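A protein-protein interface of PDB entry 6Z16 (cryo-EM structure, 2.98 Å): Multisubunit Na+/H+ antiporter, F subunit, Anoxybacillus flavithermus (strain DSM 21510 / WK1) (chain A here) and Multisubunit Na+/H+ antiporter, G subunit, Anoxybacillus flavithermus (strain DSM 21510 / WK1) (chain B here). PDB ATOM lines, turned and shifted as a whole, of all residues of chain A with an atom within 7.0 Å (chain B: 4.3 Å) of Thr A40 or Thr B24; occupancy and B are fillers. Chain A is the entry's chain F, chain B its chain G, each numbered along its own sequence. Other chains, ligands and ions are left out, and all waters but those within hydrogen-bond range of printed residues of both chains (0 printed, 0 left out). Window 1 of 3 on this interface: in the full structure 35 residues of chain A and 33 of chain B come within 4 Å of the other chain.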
ATOM      1  N   ILE A   9      15.897 -15.038  -2.571  1.00  0.00           N
ATOM      2  CA  ILE A   9      15.488 -16.330  -3.118  1.00  0.00           C
ATOM      3  C   ILE A   9      14.701 -17.141  -2.087  1.00  0.00           C
ATOM      4  O   ILE A   9      13.665 -17.738  -2.410  1.00  0.00           O
ATOM      5  CB  ILE A   9      16.727 -17.077  -3.645  1.00  0.00           C
ATOM      6  CG1 ILE A   9      17.280 -16.370  -4.878  1.00  0.00           C
ATOM      7  CG2 ILE A   9      16.399 -18.470  -4.030  1.00  0.00           C
ATOM      8  CD1 ILE A   9      18.634 -16.870  -5.299  1.00  0.00           C
ATOM      9  N   LEU A  10      15.134 -17.124  -0.821  1.00  0.00           N
ATOM     10  CA  LEU A  10      14.374 -17.800   0.231  1.00  0.00           C
ATOM     11  C   LEU A  10      13.049 -17.107   0.524  1.00  0.00           C
ATOM     12  O   LEU A  10      12.068 -17.776   0.869  1.00  0.00           O
ATOM     13  CB  LEU A  10      15.194 -17.884   1.513  1.00  0.00           C
ATOM     14  CG  LEU A  10      16.384 -18.832   1.542  1.00  0.00           C
ATOM     15  CD1 LEU A  10      17.096 -18.655   2.842  1.00  0.00           C
ATOM     16  CD2 LEU A  10      15.918 -20.257   1.395  1.00  0.00           C
ATOM     17  N   SER A  11      12.998 -15.781   0.384  1.00  0.00           N
ATOM     18  CA  SER A  11      11.755 -15.054   0.608  1.00  0.00           C
ATOM     19  C   SER A  11      10.732 -15.373  -0.473  1.00  0.00           C
ATOM     20  O   SER A  11       9.554 -15.603  -0.172  1.00  0.00           O
ATOM     21  CB  SER A  11      12.042 -13.558   0.662  1.00  0.00           C
ATOM     22  OG  SER A  11      12.927 -13.257   1.726  1.00  0.00           O
ATOM     23  N   ALA A  13      10.759 -18.141  -2.143  1.00  0.00           N
ATOM     24  CA  ALA A  13      10.396 -19.532  -1.892  1.00  0.00           C
ATOM     25  C   ALA A  13       9.325 -19.646  -0.814  1.00  0.00           C
ATOM     26  O   ALA A  13       8.394 -20.452  -0.938  1.00  0.00           O
ATOM     27  CB  ALA A  13      11.634 -20.331  -1.498  1.00  0.00           C
ATOM     28  N   MET A  14       9.437 -18.837   0.243  1.00  0.00           N
ATOM     29  CA  MET A  14       8.419 -18.813   1.289  1.00  0.00           C
ATOM     30  C   MET A  14       7.093 -18.271   0.772  1.00  0.00           C
ATOM     31  O   MET A  14       6.031 -18.752   1.180  1.00  0.00           O
ATOM     32  CB  MET A  14       8.921 -17.990   2.472  1.00  0.00           C
ATOM     33  CG  MET A  14       7.981 -17.951   3.654  1.00  0.00           C
ATOM     34  SD  MET A  14       8.669 -17.076   5.064  1.00  0.00           S
ATOM     35  CE  MET A  14       9.832 -18.299   5.647  1.00  0.00           C
ATOM     36  N   PHE A  17       5.584 -21.318  -1.026  1.00  0.00           N
ATOM     37  CA  PHE A  17       4.952 -22.244  -0.086  1.00  0.00           C
ATOM     38  C   PHE A  17       3.702 -21.634   0.537  1.00  0.00           C
ATOM     39  O   PHE A  17       2.767 -22.360   0.884  1.00  0.00           O
ATOM     40  CB  PHE A  17       5.919 -22.683   1.021  1.00  0.00           C
ATOM     41  CG  PHE A  17       7.084 -23.495   0.534  1.00  0.00           C
ATOM     42  CD1 PHE A  17       6.881 -24.733  -0.048  1.00  0.00           C
ATOM     43  CD2 PHE A  17       8.385 -23.065   0.741  1.00  0.00           C
ATOM     44  CE1 PHE A  17       7.947 -25.485  -0.491  1.00  0.00           C
ATOM     45  CE2 PHE A  17       9.457 -23.818   0.310  1.00  0.00           C
ATOM     46  CZ  PHE A  17       9.237 -25.031  -0.302  1.00  0.00           C
ATOM     47  N   ALA A  33       3.273 -27.598   3.126  1.00  0.00           N
ATOM     48  CA  ALA A  33       3.688 -26.228   2.853  1.00  0.00           C
ATOM     49  C   ALA A  33       4.109 -25.501   4.125  1.00  0.00           C
ATOM     50  O   ALA A  33       5.095 -24.756   4.116  1.00  0.00           O
ATOM     51  CB  ALA A  33       2.562 -25.479   2.149  1.00  0.00           C
ATOM     52  N   LEU A  34       3.399 -25.724   5.236  1.00  0.00           N
ATOM     53  CA  LEU A  34       3.791 -25.093   6.498  1.00  0.00           C
ATOM     54  C   LEU A  34       5.101 -25.663   7.035  1.00  0.00           C
ATOM     55  O   LEU A  34       5.919 -24.922   7.599  1.00  0.00           O
ATOM     56  CB  LEU A  34       2.678 -25.245   7.529  1.00  0.00           C
ATOM     57  CG  LEU A  34       1.472 -24.352   7.263  1.00  0.00           C
ATOM     58  CD1 LEU A  34       0.311 -24.702   8.163  1.00  0.00           C
ATOM     59  CD2 LEU A  34       1.877 -22.903   7.442  1.00  0.00           C
ATOM     60  N   ASP A  35       5.315 -26.972   6.860  1.00  0.00           N
ATOM     61  CA  ASP A  35       6.573 -27.602   7.264  1.00  0.00           C
ATOM     62  C   ASP A  35       7.757 -27.015   6.498  1.00  0.00           C
ATOM     63  O   ASP A  35       8.774 -26.619   7.094  1.00  0.00           O
ATOM     64  CB  ASP A  35       6.480 -29.109   7.034  1.00  0.00           C
ATOM     65  CG  ASP A  35       7.588 -29.888   7.726  1.00  0.00           C
ATOM     66  OD1 ASP A  35       8.442 -29.281   8.406  1.00  0.00           O
ATOM     67  OD2 ASP A  35       7.596 -31.130   7.595  1.00  0.00           O
ATOM     68  N   ALA A  36       7.630 -26.936   5.171  1.00  0.00           N
ATOM     69  CA  ALA A  36       8.690 -26.357   4.356  1.00  0.00           C
ATOM     70  C   ALA A  36       8.873 -24.872   4.627  1.00  0.00           C
ATOM     71  O   ALA A  36       9.994 -24.360   4.533  1.00  0.00           O
ATOM     72  CB  ALA A  36       8.390 -26.585   2.886  1.00  0.00           C
ATOM     73  N   MET A  37       7.795 -24.180   5.000  1.00  0.00           N
ATOM     74  CA  MET A  37       7.879 -22.764   5.323  1.00  0.00           C
ATOM     75  C   MET A  37       8.657 -22.543   6.612  1.00  0.00           C
ATOM     76  O   MET A  37       9.452 -21.601   6.714  1.00  0.00           O
ATOM     77  CB  MET A  37       6.465 -22.210   5.437  1.00  0.00           C
ATOM     78  CG  MET A  37       6.336 -20.723   5.408  1.00  0.00           C
ATOM     79  SD  MET A  37       4.594 -20.338   5.630  1.00  0.00           S
ATOM     80  CE  MET A  37       3.902 -21.131   4.190  1.00  0.00           C
ATOM     81  N   GLY A  38       8.464 -23.427   7.595  1.00  0.00           N
ATOM     82  CA  GLY A  38       9.253 -23.351   8.816  1.00  0.00           C
ATOM     83  C   GLY A  38      10.724 -23.649   8.593  1.00  0.00           C
ATOM     84  O   GLY A  38      11.596 -22.969   9.148  1.00  0.00           O
ATOM     85  N   ILE A  39      11.022 -24.654   7.765  1.00  0.00           N
ATOM     86  CA  ILE A  39      12.420 -24.966   7.463  1.00  0.00           C
ATOM     87  C   ILE A  39      13.087 -23.818   6.695  1.00  0.00           C
ATOM     88  O   ILE A  39      14.257 -23.470   6.941  1.00  0.00           O
ATOM     89  CB  ILE A  39      12.493 -26.304   6.707  1.00  0.00           C
ATOM     90  CG1 ILE A  39      11.948 -27.427   7.585  1.00  0.00           C
ATOM     91  CG2 ILE A  39      13.899 -26.648   6.343  1.00  0.00           C
ATOM     92  CD1 ILE A  39      11.782 -28.732   6.858  1.00  0.00           C
ATOM     93  N   THR A  40      12.337 -23.166   5.804  1.00  0.00           N
ATOM     94  CA  THR A  40      12.849 -21.992   5.107  1.00  0.00           C
ATOM     95  C   THR A  40      13.073 -20.825   6.066  1.00  0.00           C
ATOM     96  O   THR A  40      14.031 -20.059   5.897  1.00  0.00           O
ATOM     97  CB  THR A  40      11.877 -21.608   3.992  1.00  0.00           C
ATOM     98  OG1 THR A  40      11.623 -22.759   3.181  1.00  0.00           O
ATOM     99  CG2 THR A  40      12.463 -20.528   3.105  1.00  0.00           C
ATOM    100  N   LEU A  41      12.221 -20.700   7.090  1.00  0.00           N
ATOM    101  CA  LEU A  41      12.443 -19.709   8.141  1.00  0.00           C
ATOM    102  C   LEU A  41      13.740 -19.976   8.898  1.00  0.00           C
ATOM    103  O   LEU A  41      14.465 -19.037   9.251  1.00  0.00           O
ATOM    104  CB  LEU A  41      11.254 -19.697   9.102  1.00  0.00           C
ATOM    105  CG  LEU A  41      11.321 -18.765  10.310  1.00  0.00           C
ATOM    106  CD1 LEU A  41      11.426 -17.324   9.869  1.00  0.00           C
ATOM    107  CD2 LEU A  41      10.109 -18.969  11.197  1.00  0.00           C
ATOM    108  N   ALA A  42      14.048 -21.253   9.142  1.00  0.00           N
ATOM    109  CA  ALA A  42      15.323 -21.612   9.769  1.00  0.00           C
ATOM    110  C   ALA A  42      16.509 -21.205   8.897  1.00  0.00           C
ATOM    111  O   ALA A  42      17.535 -20.725   9.404  1.00  0.00           O
ATOM    112  CB  ALA A  42      15.367 -23.111  10.057  1.00  0.00           C
ATOM    113  N   GLY A  43      16.369 -21.364   7.580  1.00  0.00           N
ATOM    114  CA  GLY A  43      17.413 -20.892   6.676  1.00  0.00           C
ATOM    115  C   GLY A  43      17.586 -19.384   6.678  1.00  0.00           C
ATOM    116  O   GLY A  43      18.713 -18.877   6.604  1.00  0.00           O
ATOM    117  N   ILE A  44      16.470 -18.653   6.755  1.00  0.00           N
ATOM    118  CA  ILE A  44      16.515 -17.193   6.831  1.00  0.00           C
ATOM    119  C   ILE A  44      17.213 -16.745   8.109  1.00  0.00           C
ATOM    120  O   ILE A  44      18.006 -15.793   8.097  1.00  0.00           O
ATOM    121  CB  ILE A  44      15.091 -16.614   6.712  1.00  0.00           C
ATOM    122  CG1 ILE A  44      14.534 -16.882   5.319  1.00  0.00           C
ATOM    123  CG2 ILE A  44      15.059 -15.121   6.973  1.00  0.00           C
ATOM    124  CD1 ILE A  44      13.086 -16.572   5.184  1.00  0.00           C
ATOM    125  N   VAL A  45      16.970 -17.455   9.217  1.00  0.00           N
ATOM    126  CA  VAL A  45      17.632 -17.123  10.479  1.00  0.00           C
ATOM    127  C   VAL A  45      19.135 -17.383  10.389  1.00  0.00           C
ATOM    128  O   VAL A  45      19.941 -16.578  10.874  1.00  0.00           O
ATOM    129  CB  VAL A  45      16.975 -17.892  11.641  1.00  0.00           C
ATOM    130  CG1 VAL A  45      17.745 -17.701  12.933  1.00  0.00           C
ATOM    131  CG2 VAL A  45      15.568 -17.405  11.840  1.00  0.00           C
ATOM    132  N   ALA A  46      19.532 -18.471   9.714  1.00  0.00           N
ATOM    133  CA  ALA A  46      20.957 -18.749   9.511  1.00  0.00           C
ATOM    134  C   ALA A  46      21.645 -17.663   8.684  1.00  0.00           C
ATOM    135  O   ALA A  46      22.749 -17.209   9.027  1.00  0.00           O
ATOM    136  CB  ALA A  46      21.131 -20.109   8.839  1.00  0.00           C
ATOM    137  N   ILE A  64      13.753 -24.428  15.629  1.00  0.00           N
ATOM    138  CA  ILE A  64      12.773 -24.426  14.543  1.00  0.00           C
ATOM    139  C   ILE A  64      12.664 -25.813  13.922  1.00  0.00           C
ATOM    140  O   ILE A  64      11.559 -26.281  13.614  1.00  0.00           O
ATOM    141  CB  ILE A  64      13.134 -23.344  13.506  1.00  0.00           C
ATOM    142  CG1 ILE A  64      12.861 -21.955  14.066  1.00  0.00           C
ATOM    143  CG2 ILE A  64      12.333 -23.502  12.256  1.00  0.00           C
ATOM    144  CD1 ILE A  64      13.505 -20.870  13.271  1.00  0.00           C
ATOM    145  N   GLY B  20      22.133 -23.833  -1.871  1.00  0.00           N
ATOM    146  CA  GLY B  20      21.039 -24.162  -0.969  1.00  0.00           C
ATOM    147  C   GLY B  20      19.829 -23.268  -1.158  1.00  0.00           C
ATOM    148  O   GLY B  20      18.688 -23.744  -1.137  1.00  0.00           O
ATOM    149  N   ALA B  21      20.064 -21.972  -1.402  1.00  0.00           N
ATOM    150  CA  ALA B  21      18.960 -21.046  -1.651  1.00  0.00           C
ATOM    151  C   ALA B  21      18.208 -21.390  -2.939  1.00  0.00           C
ATOM    152  O   ALA B  21      16.970 -21.485  -2.942  1.00  0.00           O
ATOM    153  CB  ALA B  21      19.490 -19.614  -1.697  1.00  0.00           C
ATOM    154  N   VAL B  22      18.945 -21.602  -4.038  1.00  0.00           N
ATOM    155  CA  VAL B  22      18.336 -21.922  -5.331  1.00  0.00           C
ATOM    156  C   VAL B  22      17.611 -23.261  -5.271  1.00  0.00           C
ATOM    157  O   VAL B  22      16.529 -23.427  -5.850  1.00  0.00           O
ATOM    158  CB  VAL B  22      19.414 -21.887  -6.434  1.00  0.00           C
ATOM    159  CG1 VAL B  22      18.910 -22.449  -7.744  1.00  0.00           C
ATOM    160  CG2 VAL B  22      19.872 -20.462  -6.657  1.00  0.00           C
ATOM    161  N   LEU B  23      18.147 -24.209  -4.509  1.00  0.00           N
ATOM    162  CA  LEU B  23      17.506 -25.509  -4.408  1.00  0.00           C
ATOM    163  C   LEU B  23      16.241 -25.442  -3.552  1.00  0.00           C
ATOM    164  O   LEU B  23      15.272 -26.171  -3.810  1.00  0.00           O
ATOM    165  CB  LEU B  23      18.535 -26.489  -3.864  1.00  0.00           C
ATOM    166  CG  LEU B  23      18.368 -27.988  -3.937  1.00  0.00           C
ATOM    167  CD1 LEU B  23      18.183 -28.377  -5.376  1.00  0.00           C
ATOM    168  CD2 LEU B  23      19.663 -28.556  -3.417  1.00  0.00           C
ATOM    169  N   THR B  24      16.201 -24.521  -2.582  1.00  0.00           N
ATOM    170  CA  THR B  24      14.960 -24.277  -1.847  1.00  0.00           C
ATOM    171  C   THR B  24      13.900 -23.628  -2.739  1.00  0.00           C
ATOM    172  O   THR B  24      12.713 -23.977  -2.664  1.00  0.00           O
ATOM    173  CB  THR B  24      15.250 -23.404  -0.629  1.00  0.00           C
ATOM    174  OG1 THR B  24      16.310 -23.996   0.126  1.00  0.00           O
ATOM    175  CG2 THR B  24      14.035 -23.314   0.266  1.00  0.00           C
ATOM    176  N   LEU B  25      14.313 -22.692  -3.600  1.00  0.00           N
ATOM    177  CA  LEU B  25      13.373 -22.098  -4.555  1.00  0.00           C
ATOM    178  C   LEU B  25      12.866 -23.122  -5.561  1.00  0.00           C
ATOM    179  O   LEU B  25      11.712 -23.047  -6.004  1.00  0.00           O
ATOM    180  CB  LEU B  25      14.028 -20.935  -5.289  1.00  0.00           C
ATOM    181  CG  LEU B  25      13.197 -20.099  -6.263  1.00  0.00           C
ATOM    182  CD1 LEU B  25      12.047 -19.417  -5.549  1.00  0.00           C
ATOM    183  CD2 LEU B  25      14.080 -19.074  -6.945  1.00  0.00           C
ATOM    184  N   LEU B  26      13.711 -24.085  -5.922  1.00  0.00           N
ATOM    185  CA  LEU B  26      13.277 -25.196  -6.758  1.00  0.00           C
ATOM    186  C   LEU B  26      12.250 -26.063  -6.042  1.00  0.00           C
ATOM    187  O   LEU B  26      11.291 -26.538  -6.664  1.00  0.00           O
ATOM    188  CB  LEU B  26      14.485 -26.023  -7.174  1.00  0.00           C
ATOM    189  CG  LEU B  26      14.235 -27.268  -8.009  1.00  0.00           C
ATOM    190  CD1 LEU B  26      13.614 -26.926  -9.351  1.00  0.00           C
ATOM    191  CD2 LEU B  26      15.553 -27.958  -8.175  1.00  0.00           C
ATOM    192  N   SER B  27      12.430 -26.263  -4.733  1.00  0.00           N
ATOM    193  CA  SER B  27      11.410 -26.947  -3.937  1.00  0.00           C
ATOM    194  C   SER B  27      10.091 -26.182  -3.940  1.00  0.00           C
ATOM    195  O   SER B  27       9.014 -26.783  -3.989  1.00  0.00           O
ATOM    196  CB  SER B  27      11.899 -27.137  -2.505  1.00  0.00           C
ATOM    197  OG  SER B  27      10.892 -27.723  -1.705  1.00  0.00           O
ATOM    198  N   ALA B  28      10.163 -24.850  -3.922  1.00  0.00           N
ATOM    199  CA  ALA B  28       8.943 -24.041  -3.914  1.00  0.00           C
ATOM    200  C   ALA B  28       8.212 -24.090  -5.253  1.00  0.00           C
ATOM    201  O   ALA B  28       6.979 -24.217  -5.291  1.00  0.00           O
ATOM    202  CB  ALA B  28       9.280 -22.604  -3.554  1.00  0.00           C
ATOM    203  N   THR B  48      13.929 -29.409  -0.376  1.00  0.00           N
ATOM    204  CA  THR B  48      14.195 -28.456   0.691  1.00  0.00           C
ATOM    205  C   THR B  48      15.041 -29.071   1.798  1.00  0.00           C
ATOM    206  O   THR B  48      15.745 -28.316   2.476  1.00  0.00           O
ATOM    207  CB  THR B  48      12.905 -27.841   1.266  1.00  0.00           C
ATOM    208  OG1 THR B  48      13.218 -26.553   1.804  1.00  0.00           O
ATOM    209  CG2 THR B  48      12.335 -28.648   2.426  1.00  0.00           C
ATOM    210  N   GLY B  51      18.501 -28.487   0.374  1.00  0.00           N
ATOM    211  CA  GLY B  51      18.749 -27.053   0.357  1.00  0.00           C
ATOM    212  C   GLY B  51      19.084 -26.489   1.725  1.00  0.00           C
ATOM    213  O   GLY B  51      20.044 -25.723   1.873  1.00  0.00           O
ATOM    214  N   ILE B  55      22.654 -24.814   3.085  1.00  0.00           N
ATOM    215  CA  ILE B  55      22.716 -23.494   3.720  1.00  0.00           C
ATOM    216  C   ILE B  55      23.375 -23.578   5.096  1.00  0.00           C
ATOM    217  O   ILE B  55      24.224 -22.743   5.449  1.00  0.00           O
ATOM    218  CB  ILE B  55      21.306 -22.875   3.801  1.00  0.00           C
ATOM    219  CG1 ILE B  55      20.763 -22.591   2.407  1.00  0.00           C
ATOM    220  CG2 ILE B  55      21.314 -21.579   4.580  1.00  0.00           C
ATOM    221  CD1 ILE B  55      19.288 -22.285   2.393  1.00  0.00           C
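The backbone carbonyl oxygen (O) of Ala A36 is in hydrogen-bond range of the side-chain hydroxyl (OG1) of Thr A40. The side-chain hydroxyl (OG1) of Thr B24 lies within hydrogen-bond range of the backbone carbonyl oxygen (O) of Gly B20, at 2.7 Å.
Ile A9 touches Ala B21 (CG2 to O, 3.3 Å). Leu B25 touches Ile A9. Leu A10 touches Thr B24 (CD2 to CG2, 3.8 Å). Ala A13 touches Thr B24. Ala A13 touches Leu B25 (N to CD1, 3.9 Å). Ala A13 touches Ala B28 (O to CB, 3.5 Å). Ser B27 touches Phe A17 (OG to CZ, 3.5 Å). N of Ala B28 touches CZ of Phe A17 (3.7 Å). Thr A40 touches Thr B24 (OG1 to CG2, 3.8 Å).
Of the printed residues of chain B, Ala A13 touches Thr B24, Leu B25 and Ala B28. Printed residues of chain B within 4 Å of Phe A17: Ser B27 and Ala B28. Printed residues of chain A within 4 Å of Leu B25: Ile A9 and Ala A13. The nearest printed residue of chain B that does not touch Thr A40 is Thr B48 (4.3 Å). The nearest residue of chain A that does not touch Thr B24 is Phe A17 (4.3 Å). The nearest printed residue of chain A that does not touch Leu B25 is Leu A10 (5.8 Å).
Of the 12 printed residues of chain B, 5 touch a printed residue of chain A. Hydrophobic or aromatic side chains of chain A that line the printed part of chain B: Ile A9, Leu A10, Ala A13 and Phe A17. Among the printed residues, 9 pairs touch across the chains. Among the printed residues, no Asp or Glu carboxylate lies within 4 Å of a Lys or Arg side-chain nitrogen of the other chain.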
